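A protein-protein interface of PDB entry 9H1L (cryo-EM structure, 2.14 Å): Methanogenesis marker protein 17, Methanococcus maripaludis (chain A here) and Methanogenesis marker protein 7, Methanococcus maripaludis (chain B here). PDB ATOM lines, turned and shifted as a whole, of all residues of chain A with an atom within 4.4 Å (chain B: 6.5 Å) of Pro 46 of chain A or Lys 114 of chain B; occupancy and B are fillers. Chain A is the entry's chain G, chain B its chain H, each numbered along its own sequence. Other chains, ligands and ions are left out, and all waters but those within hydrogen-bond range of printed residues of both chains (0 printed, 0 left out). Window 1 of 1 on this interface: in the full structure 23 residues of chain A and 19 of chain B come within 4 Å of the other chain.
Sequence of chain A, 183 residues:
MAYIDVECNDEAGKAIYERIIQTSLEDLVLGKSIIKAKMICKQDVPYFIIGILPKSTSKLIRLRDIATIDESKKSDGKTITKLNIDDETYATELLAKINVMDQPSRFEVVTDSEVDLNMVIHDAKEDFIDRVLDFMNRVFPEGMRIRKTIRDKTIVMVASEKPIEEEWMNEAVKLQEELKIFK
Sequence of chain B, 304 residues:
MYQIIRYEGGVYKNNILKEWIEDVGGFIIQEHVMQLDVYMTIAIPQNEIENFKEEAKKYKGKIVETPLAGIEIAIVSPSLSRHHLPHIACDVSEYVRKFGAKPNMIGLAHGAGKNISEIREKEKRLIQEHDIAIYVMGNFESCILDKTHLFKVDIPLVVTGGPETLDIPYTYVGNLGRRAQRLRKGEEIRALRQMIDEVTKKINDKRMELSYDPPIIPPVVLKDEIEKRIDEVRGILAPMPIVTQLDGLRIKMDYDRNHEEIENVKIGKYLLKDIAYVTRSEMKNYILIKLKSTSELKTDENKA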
ATOM      1  N   LYS A  42       0.642 -19.396  -7.691  1.00  0.00           N
ATOM      2  CA  LYS A  42      -0.800 -19.519  -7.866  1.00  0.00           C
ATOM      3  C   LYS A  42      -1.038 -20.765  -8.710  1.00  0.00           C
ATOM      4  O   LYS A  42      -0.742 -20.774  -9.908  1.00  0.00           O
ATOM      5  CB  LYS A  42      -1.386 -18.276  -8.526  1.00  0.00           C
ATOM      6  CG  LYS A  42      -1.148 -16.994  -7.749  1.00  0.00           C
ATOM      7  CD  LYS A  42      -2.445 -16.434  -7.195  1.00  0.00           C
ATOM      8  CE  LYS A  42      -2.221 -15.740  -5.864  1.00  0.00           C
ATOM      9  NZ  LYS A  42      -2.322 -16.689  -4.721  1.00  0.00           N
ATOM     10  N   GLN A  43      -1.550 -21.825  -8.079  1.00  0.00           N
ATOM     11  CA  GLN A  43      -1.733 -23.098  -8.753  1.00  0.00           C
ATOM     12  C   GLN A  43      -3.185 -23.437  -9.056  1.00  0.00           C
ATOM     13  O   GLN A  43      -3.431 -24.304  -9.899  1.00  0.00           O
ATOM     14  CB  GLN A  43      -1.119 -24.237  -7.924  1.00  0.00           C
ATOM     15  CG  GLN A  43      -1.774 -24.443  -6.571  1.00  0.00           C
ATOM     16  CD  GLN A  43      -1.030 -23.741  -5.456  1.00  0.00           C
ATOM     17  OE1 GLN A  43      -0.229 -22.842  -5.704  1.00  0.00           O
ATOM     18  NE2 GLN A  43      -1.292 -24.146  -4.221  1.00  0.00           N
ATOM     19  N   ASP A  44      -4.142 -22.795  -8.383  1.00  0.00           N
ATOM     20  CA  ASP A  44      -5.549 -23.011  -8.706  1.00  0.00           C
ATOM     21  C   ASP A  44      -5.866 -22.499 -10.107  1.00  0.00           C
ATOM     22  O   ASP A  44      -6.498 -23.195 -10.907  1.00  0.00           O
ATOM     23  CB  ASP A  44      -6.433 -22.334  -7.662  1.00  0.00           C
ATOM     24  CG  ASP A  44      -5.892 -22.495  -6.255  1.00  0.00           C
ATOM     25  OD1 ASP A  44      -5.097 -21.636  -5.819  1.00  0.00           O
ATOM     26  OD2 ASP A  44      -6.256 -23.486  -5.587  1.00  0.00           O
ATOM     27  N   VAL A  45      -5.427 -21.286 -10.415  1.00  0.00           N
ATOM     28  CA  VAL A  45      -5.290 -20.806 -11.785  1.00  0.00           C
ATOM     29  C   VAL A  45      -3.800 -20.812 -12.109  1.00  0.00           C
ATOM     30  O   VAL A  45      -3.025 -20.120 -11.435  1.00  0.00           O
ATOM     31  CB  VAL A  45      -5.911 -19.411 -11.976  1.00  0.00           C
ATOM     32  CG1 VAL A  45      -5.713 -18.538 -10.737  1.00  0.00           C
ATOM     33  CG2 VAL A  45      -5.358 -18.732 -13.226  1.00  0.00           C
ATOM     34  N   PRO A  46      -3.349 -21.600 -13.087  1.00  0.00           N
ATOM     35  CA  PRO A  46      -1.903 -21.819 -13.240  1.00  0.00           C
ATOM     36  C   PRO A  46      -1.161 -20.602 -13.764  1.00  0.00           C
ATOM     37  O   PRO A  46      -1.209 -20.296 -14.960  1.00  0.00           O
ATOM     38  CB  PRO A  46      -1.828 -22.987 -14.234  1.00  0.00           C
ATOM     39  CG  PRO A  46      -3.211 -23.563 -14.288  1.00  0.00           C
ATOM     40  CD  PRO A  46      -4.134 -22.430 -14.010  1.00  0.00           C
ATOM     41  N   TYR A  47      -0.456 -19.922 -12.861  1.00  0.00           N
ATOM     42  CA  TYR A  47       0.391 -18.784 -13.195  1.00  0.00           C
ATOM     43  C   TYR A  47       1.347 -18.575 -12.031  1.00  0.00           C
ATOM     44  O   TYR A  47       0.925 -18.595 -10.871  1.00  0.00           O
ATOM     45  CB  TYR A  47      -0.471 -17.533 -13.520  1.00  0.00           C
ATOM     46  CG  TYR A  47      -0.818 -16.535 -12.415  1.00  0.00           C
ATOM     47  CD1 TYR A  47       0.115 -15.625 -11.915  1.00  0.00           C
ATOM     48  CD2 TYR A  47      -2.102 -16.505 -11.882  1.00  0.00           C
ATOM     49  CE1 TYR A  47      -0.224 -14.730 -10.921  1.00  0.00           C
ATOM     50  CE2 TYR A  47      -2.445 -15.613 -10.887  1.00  0.00           C
ATOM     51  CZ  TYR A  47      -1.503 -14.727 -10.413  1.00  0.00           C
ATOM     52  OH  TYR A  47      -1.844 -13.839  -9.419  1.00  0.00           O
ATOM     53  N   MET A 144       4.247 -24.340 -17.631  1.00  0.00           N
ATOM     54  CA  MET A 144       4.142 -22.884 -17.700  1.00  0.00           C
ATOM     55  C   MET A 144       5.141 -22.387 -18.743  1.00  0.00           C
ATOM     56  O   MET A 144       6.251 -21.948 -18.438  1.00  0.00           O
ATOM     57  CB  MET A 144       4.390 -22.271 -16.328  1.00  0.00           C
ATOM     58  CG  MET A 144       3.511 -22.845 -15.231  1.00  0.00           C
ATOM     59  SD  MET A 144       1.995 -23.595 -15.852  1.00  0.00           S
ATOM     60  CE  MET A 144       1.534 -24.631 -14.467  1.00  0.00           C
ATOM     61  N   SER A 160       2.956 -19.011 -17.385  1.00  0.00           N
ATOM     62  CA  SER A 160       1.649 -19.649 -17.343  1.00  0.00           C
ATOM     63  C   SER A 160       1.487 -20.545 -18.563  1.00  0.00           C
ATOM     64  O   SER A 160       2.183 -20.391 -19.570  1.00  0.00           O
ATOM     65  CB  SER A 160       0.521 -18.617 -17.293  1.00  0.00           C
ATOM     66  OG  SER A 160      -0.700 -19.216 -16.897  1.00  0.00           O
ATOM     67  N   GLU A 161       0.558 -21.496 -18.454  1.00  0.00           N
ATOM     68  CA  GLU A 161       0.183 -22.315 -19.602  1.00  0.00           C
ATOM     69  C   GLU A 161      -0.830 -21.620 -20.497  1.00  0.00           C
ATOM     70  O   GLU A 161      -1.033 -22.052 -21.638  1.00  0.00           O
ATOM     71  CB  GLU A 161      -0.382 -23.656 -19.133  1.00  0.00           C
ATOM     72  CG  GLU A 161      -1.172 -23.576 -17.842  1.00  0.00           C
ATOM     73  CD  GLU A 161      -2.007 -24.817 -17.595  1.00  0.00           C
ATOM     74  OE1 GLU A 161      -1.443 -25.843 -17.160  1.00  0.00           O
ATOM     75  OE2 GLU A 161      -3.233 -24.764 -17.831  1.00  0.00           O
ATOM     76  N   LYS A 162      -1.462 -20.566 -20.008  1.00  0.00           N
ATOM     77  CA  LYS A 162      -2.396 -19.716 -20.725  1.00  0.00           C
ATOM     78  C   LYS A 162      -1.721 -18.409 -21.114  1.00  0.00           C
ATOM     79  O   LYS A 162      -0.654 -18.075 -20.588  1.00  0.00           O
ATOM     80  CB  LYS A 162      -3.626 -19.432 -19.850  1.00  0.00           C
ATOM     81  CG  LYS A 162      -4.342 -20.676 -19.365  1.00  0.00           C
ATOM     82  CD  LYS A 162      -5.518 -20.317 -18.475  1.00  0.00           C
ATOM     83  CE  LYS A 162      -5.187 -20.527 -17.010  1.00  0.00           C
ATOM     84  NZ  LYS A 162      -6.327 -21.138 -16.273  1.00  0.00           N
ATOM     85  N   ALA B 112       3.030 -32.635 -19.121  1.00  0.00           N
ATOM     86  CA  ALA B 112       3.265 -31.429 -18.344  1.00  0.00           C
ATOM     87  C   ALA B 112       2.066 -30.497 -18.432  1.00  0.00           C
ATOM     88  O   ALA B 112       1.303 -30.526 -19.402  1.00  0.00           O
ATOM     89  CB  ALA B 112       4.524 -30.701 -18.826  1.00  0.00           C
ATOM     90  N   GLY B 113       1.906 -29.672 -17.408  1.00  0.00           N
ATOM     91  CA  GLY B 113       0.798 -28.744 -17.314  1.00  0.00           C
ATOM     92  C   GLY B 113      -0.285 -29.252 -16.378  1.00  0.00           C
ATOM     93  O   GLY B 113      -0.280 -30.397 -15.926  1.00  0.00           O
ATOM     94  N   LYS B 114      -1.227 -28.360 -16.087  1.00  0.00           N
ATOM     95  CA  LYS B 114      -2.339 -28.681 -15.201  1.00  0.00           C
ATOM     96  C   LYS B 114      -3.596 -29.089 -15.955  1.00  0.00           C
ATOM     97  O   LYS B 114      -4.208 -30.107 -15.622  1.00  0.00           O
ATOM     98  CB  LYS B 114      -2.656 -27.491 -14.293  1.00  0.00           C
ATOM     99  CG  LYS B 114      -3.516 -27.845 -13.097  1.00  0.00           C
ATOM    100  CD  LYS B 114      -3.880 -26.610 -12.300  1.00  0.00           C
ATOM    101  CE  LYS B 114      -5.152 -26.828 -11.502  1.00  0.00           C
ATOM    102  NZ  LYS B 114      -5.131 -26.064 -10.231  1.00  0.00           N
ATOM    103  N   ASN B 115      -3.996 -28.318 -16.967  1.00  0.00           N
ATOM    104  CA  ASN B 115      -5.166 -28.632 -17.766  1.00  0.00           C
ATOM    105  C   ASN B 115      -4.835 -29.025 -19.196  1.00  0.00           C
ATOM    106  O   ASN B 115      -5.711 -29.554 -19.890  1.00  0.00           O
ATOM    107  CB  ASN B 115      -6.135 -27.440 -17.789  1.00  0.00           C
ATOM    108  CG  ASN B 115      -6.319 -26.815 -16.422  1.00  0.00           C
ATOM    109  OD1 ASN B 115      -6.599 -27.505 -15.444  1.00  0.00           O
ATOM    110  ND2 ASN B 115      -6.157 -25.499 -16.346  1.00  0.00           N
ATOM    111  N   ILE B 116      -3.607 -28.789 -19.656  1.00  0.00           N
ATOM    112  CA  ILE B 116      -3.194 -29.152 -21.003  1.00  0.00           C
ATOM    113  C   ILE B 116      -2.546 -30.532 -21.047  1.00  0.00           C
ATOM    114  O   ILE B 116      -2.020 -30.930 -22.086  1.00  0.00           O
ATOM    115  CB  ILE B 116      -2.254 -28.090 -21.595  1.00  0.00           C
ATOM    116  CG1 ILE B 116      -1.066 -27.853 -20.664  1.00  0.00           C
ATOM    117  CG2 ILE B 116      -3.004 -26.792 -21.837  1.00  0.00           C
ATOM    118  CD1 ILE B 116       0.135 -27.242 -21.349  1.00  0.00           C
ATOM    119  N   SER B 117      -2.573 -31.264 -19.938  1.00  0.00           N
ATOM    120  CA  SER B 117      -1.953 -32.579 -19.882  1.00  0.00           C
ATOM    121  C   SER B 117      -2.820 -33.616 -20.584  1.00  0.00           C
ATOM    122  O   SER B 117      -4.052 -33.578 -20.504  1.00  0.00           O
ATOM    123  CB  SER B 117      -1.713 -32.994 -18.433  1.00  0.00           C
ATOM    124  OG  SER B 117      -2.915 -32.973 -17.688  1.00  0.00           O
ATOM    125  N   SER B 142      -3.814 -29.222  -5.981  1.00  0.00           N
ATOM    126  CA  SER B 142      -4.803 -28.986  -7.026  1.00  0.00           C
ATOM    127  C   SER B 142      -4.306 -29.431  -8.393  1.00  0.00           C
ATOM    128  O   SER B 142      -5.105 -29.894  -9.219  1.00  0.00           O
ATOM    129  CB  SER B 142      -5.188 -27.507  -7.057  1.00  0.00           C
ATOM    130  OG  SER B 142      -4.441 -26.812  -8.039  1.00  0.00           O
ATOM    131  N   CYS B 143      -3.000 -29.305  -8.644  1.00  0.00           N
ATOM    132  CA  CYS B 143      -2.435 -29.720  -9.925  1.00  0.00           C
ATOM    133  C   CYS B 143      -2.591 -31.219 -10.142  1.00  0.00           C
ATOM    134  O   CYS B 143      -3.021 -31.660 -11.212  1.00  0.00           O
ATOM    135  CB  CYS B 143      -0.960 -29.318 -10.005  1.00  0.00           C
ATOM    136  SG  CYS B 143      -0.663 -27.571 -10.342  1.00  0.00           S
ATOM    137  N   ILE B 144      -2.251 -32.020  -9.129  1.00  0.00           N
ATOM    138  CA  ILE B 144      -2.381 -33.467  -9.262  1.00  0.00           C
ATOM    139  C   ILE B 144      -3.842 -33.892  -9.198  1.00  0.00           C
ATOM    140  O   ILE B 144      -4.243 -34.855  -9.863  1.00  0.00           O
ATOM    141  CB  ILE B 144      -1.532 -34.188  -8.195  1.00  0.00           C
ATOM    142  CG1 ILE B 144      -0.127 -33.592  -8.139  1.00  0.00           C
ATOM    143  CG2 ILE B 144      -1.412 -35.665  -8.519  1.00  0.00           C
ATOM    144  CD1 ILE B 144       0.675 -34.049  -6.944  1.00  0.00           C
ATOM    145  N   ASP B 146      -6.343 -32.270 -10.406  1.00  0.00           N
ATOM    146  CA  ASP B 146      -6.853 -32.030 -11.748  1.00  0.00           C
ATOM    147  C   ASP B 146      -6.082 -32.807 -12.812  1.00  0.00           C
ATOM    148  O   ASP B 146      -6.103 -32.426 -13.987  1.00  0.00           O
ATOM    149  CB  ASP B 146      -6.822 -30.532 -12.062  1.00  0.00           C
ATOM    150  CG  ASP B 146      -8.111 -30.045 -12.692  1.00  0.00           C
ATOM    151  OD1 ASP B 146      -9.173 -30.639 -12.413  1.00  0.00           O
ATOM    152  OD2 ASP B 146      -8.067 -29.065 -13.466  1.00  0.00           O
ATOM    153  N   LYS B 147      -5.407 -33.891 -12.422  1.00  0.00           N
ATOM    154  CA  LYS B 147      -4.547 -34.661 -13.312  1.00  0.00           C
ATOM    155  C   LYS B 147      -4.743 -36.158 -13.098  1.00  0.00           C
ATOM    156  O   LYS B 147      -3.819 -36.947 -13.323  1.00  0.00           O
ATOM    157  CB  LYS B 147      -3.083 -34.276 -13.098  1.00  0.00           C
ATOM    158  CG  LYS B 147      -2.220 -34.274 -14.338  1.00  0.00           C
ATOM    159  CD  LYS B 147      -0.790 -33.931 -13.970  1.00  0.00           C
ATOM    160  CE  LYS B 147       0.015 -33.526 -15.183  1.00  0.00           C
ATOM    161  NZ  LYS B 147       1.226 -32.745 -14.814  1.00  0.00           N
ATOM    162  N   HIS B 149      -6.642 -38.230 -14.748  1.00  0.00           N
ATOM    163  CA  HIS B 149      -6.799 -38.969 -16.000  1.00  0.00           C
ATOM    164  C   HIS B 149      -5.492 -39.554 -16.529  1.00  0.00           C
ATOM    165  O   HIS B 149      -5.534 -40.442 -17.387  1.00  0.00           O
ATOM    166  CB  HIS B 149      -7.412 -38.061 -17.066  1.00  0.00           C
ATOM    167  CG  HIS B 149      -6.480 -36.998 -17.562  1.00  0.00           C
ATOM    168  ND1 HIS B 149      -5.963 -36.017 -16.745  1.00  0.00           N
ATOM    169  CD2 HIS B 149      -5.970 -36.766 -18.795  1.00  0.00           C
ATOM    170  CE1 HIS B 149      -5.176 -35.227 -17.452  1.00  0.00           C
ATOM    171  NE2 HIS B 149      -5.163 -35.659 -18.699  1.00  0.00           N
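Printed residues of chain B within 4 Å of Asp 44 of chain A: Lys 114.
Printed residues of chain B within 4 Å of Glu 161 of chain A: Gly 113, Lys 114 and Asn 115.
Lys 114 of chain B touches just these residues of chain A: Gln 43 (2.5 Å), Asp 44 (3.2 Å), Pro 46 (3.7 Å) and Glu 161 (2.7 Å).
Of the printed residues of chain A, Asn 115 of chain B touches Glu 161 (3.4 Å).
The nearest residue of chain B that does not touch Pro 46 of chain A is Asn 115 of chain B (4.1 Å).
The nearest printed residue of chain B that does not touch Asp 44 of chain A is Ser 142 of chain B (4.01 Å).
Pro 46 of chain A touches Lys 114 of chain B (CG to CD, 3.7 Å).
OE1 of Glu 161 of chain A touches CA of Gly 113 of chain B (3.7 Å).
Of the 12 printed residues of chain B, 4 touch a printed residue of chain A.
Printed residues of chain A that touch a printed residue of chain B: Gln 43, Asp 44, Pro 46 and Glu 161.
Hydrophobic or aromatic side chains of chain A within 4 Å of the printed part of chain B: Pro 46.
Among the printed residues, 7 pairs touch across the chains.
The side-chain amino group (NZ) of Lys 114 of chain B lies within hydrogen-bond range of the backbone carbonyl oxygen (O) of Gln 43 of chain A (2.5 Å).
O of Gln 43 of chain A sits at hydrogen-bond distance from OG of Ser 142 of chain B, at 3.3 Å.
O of Asp 44 of chain A sits at hydrogen-bond distance from NZ of Lys 114 of chain B.
N of Lys 114 of chain B is in hydrogen-bond range of OE1 of Glu 161 of chain A, 2.7 Å away.
The side-chain amide nitrogen of Asn 115 of chain B lies within hydrogen-bond range of the side-chain carboxylate of Glu 161 of chain A (3.4 Å).
The side-chain sulfur (SD) of Met 144 of chain A is in hydrogen-bond range of the backbone NH (N) of Glu 161 of chain A, at 3.6 Å.
O of Gly 113 of chain B is in hydrogen-bond range of NZ of Lys 147 of chain B (3.0 Å).
OG of Ser 142 of chain B is in hydrogen-bond range of NZ of Lys 114 of chain B (2.4 Å).
The side-chain amide oxygen (OD1) of Asn 115 of chain B lies close to the side-chain carboxylate (OD2) of Asp 146 of chain B, 2.9 Å away.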
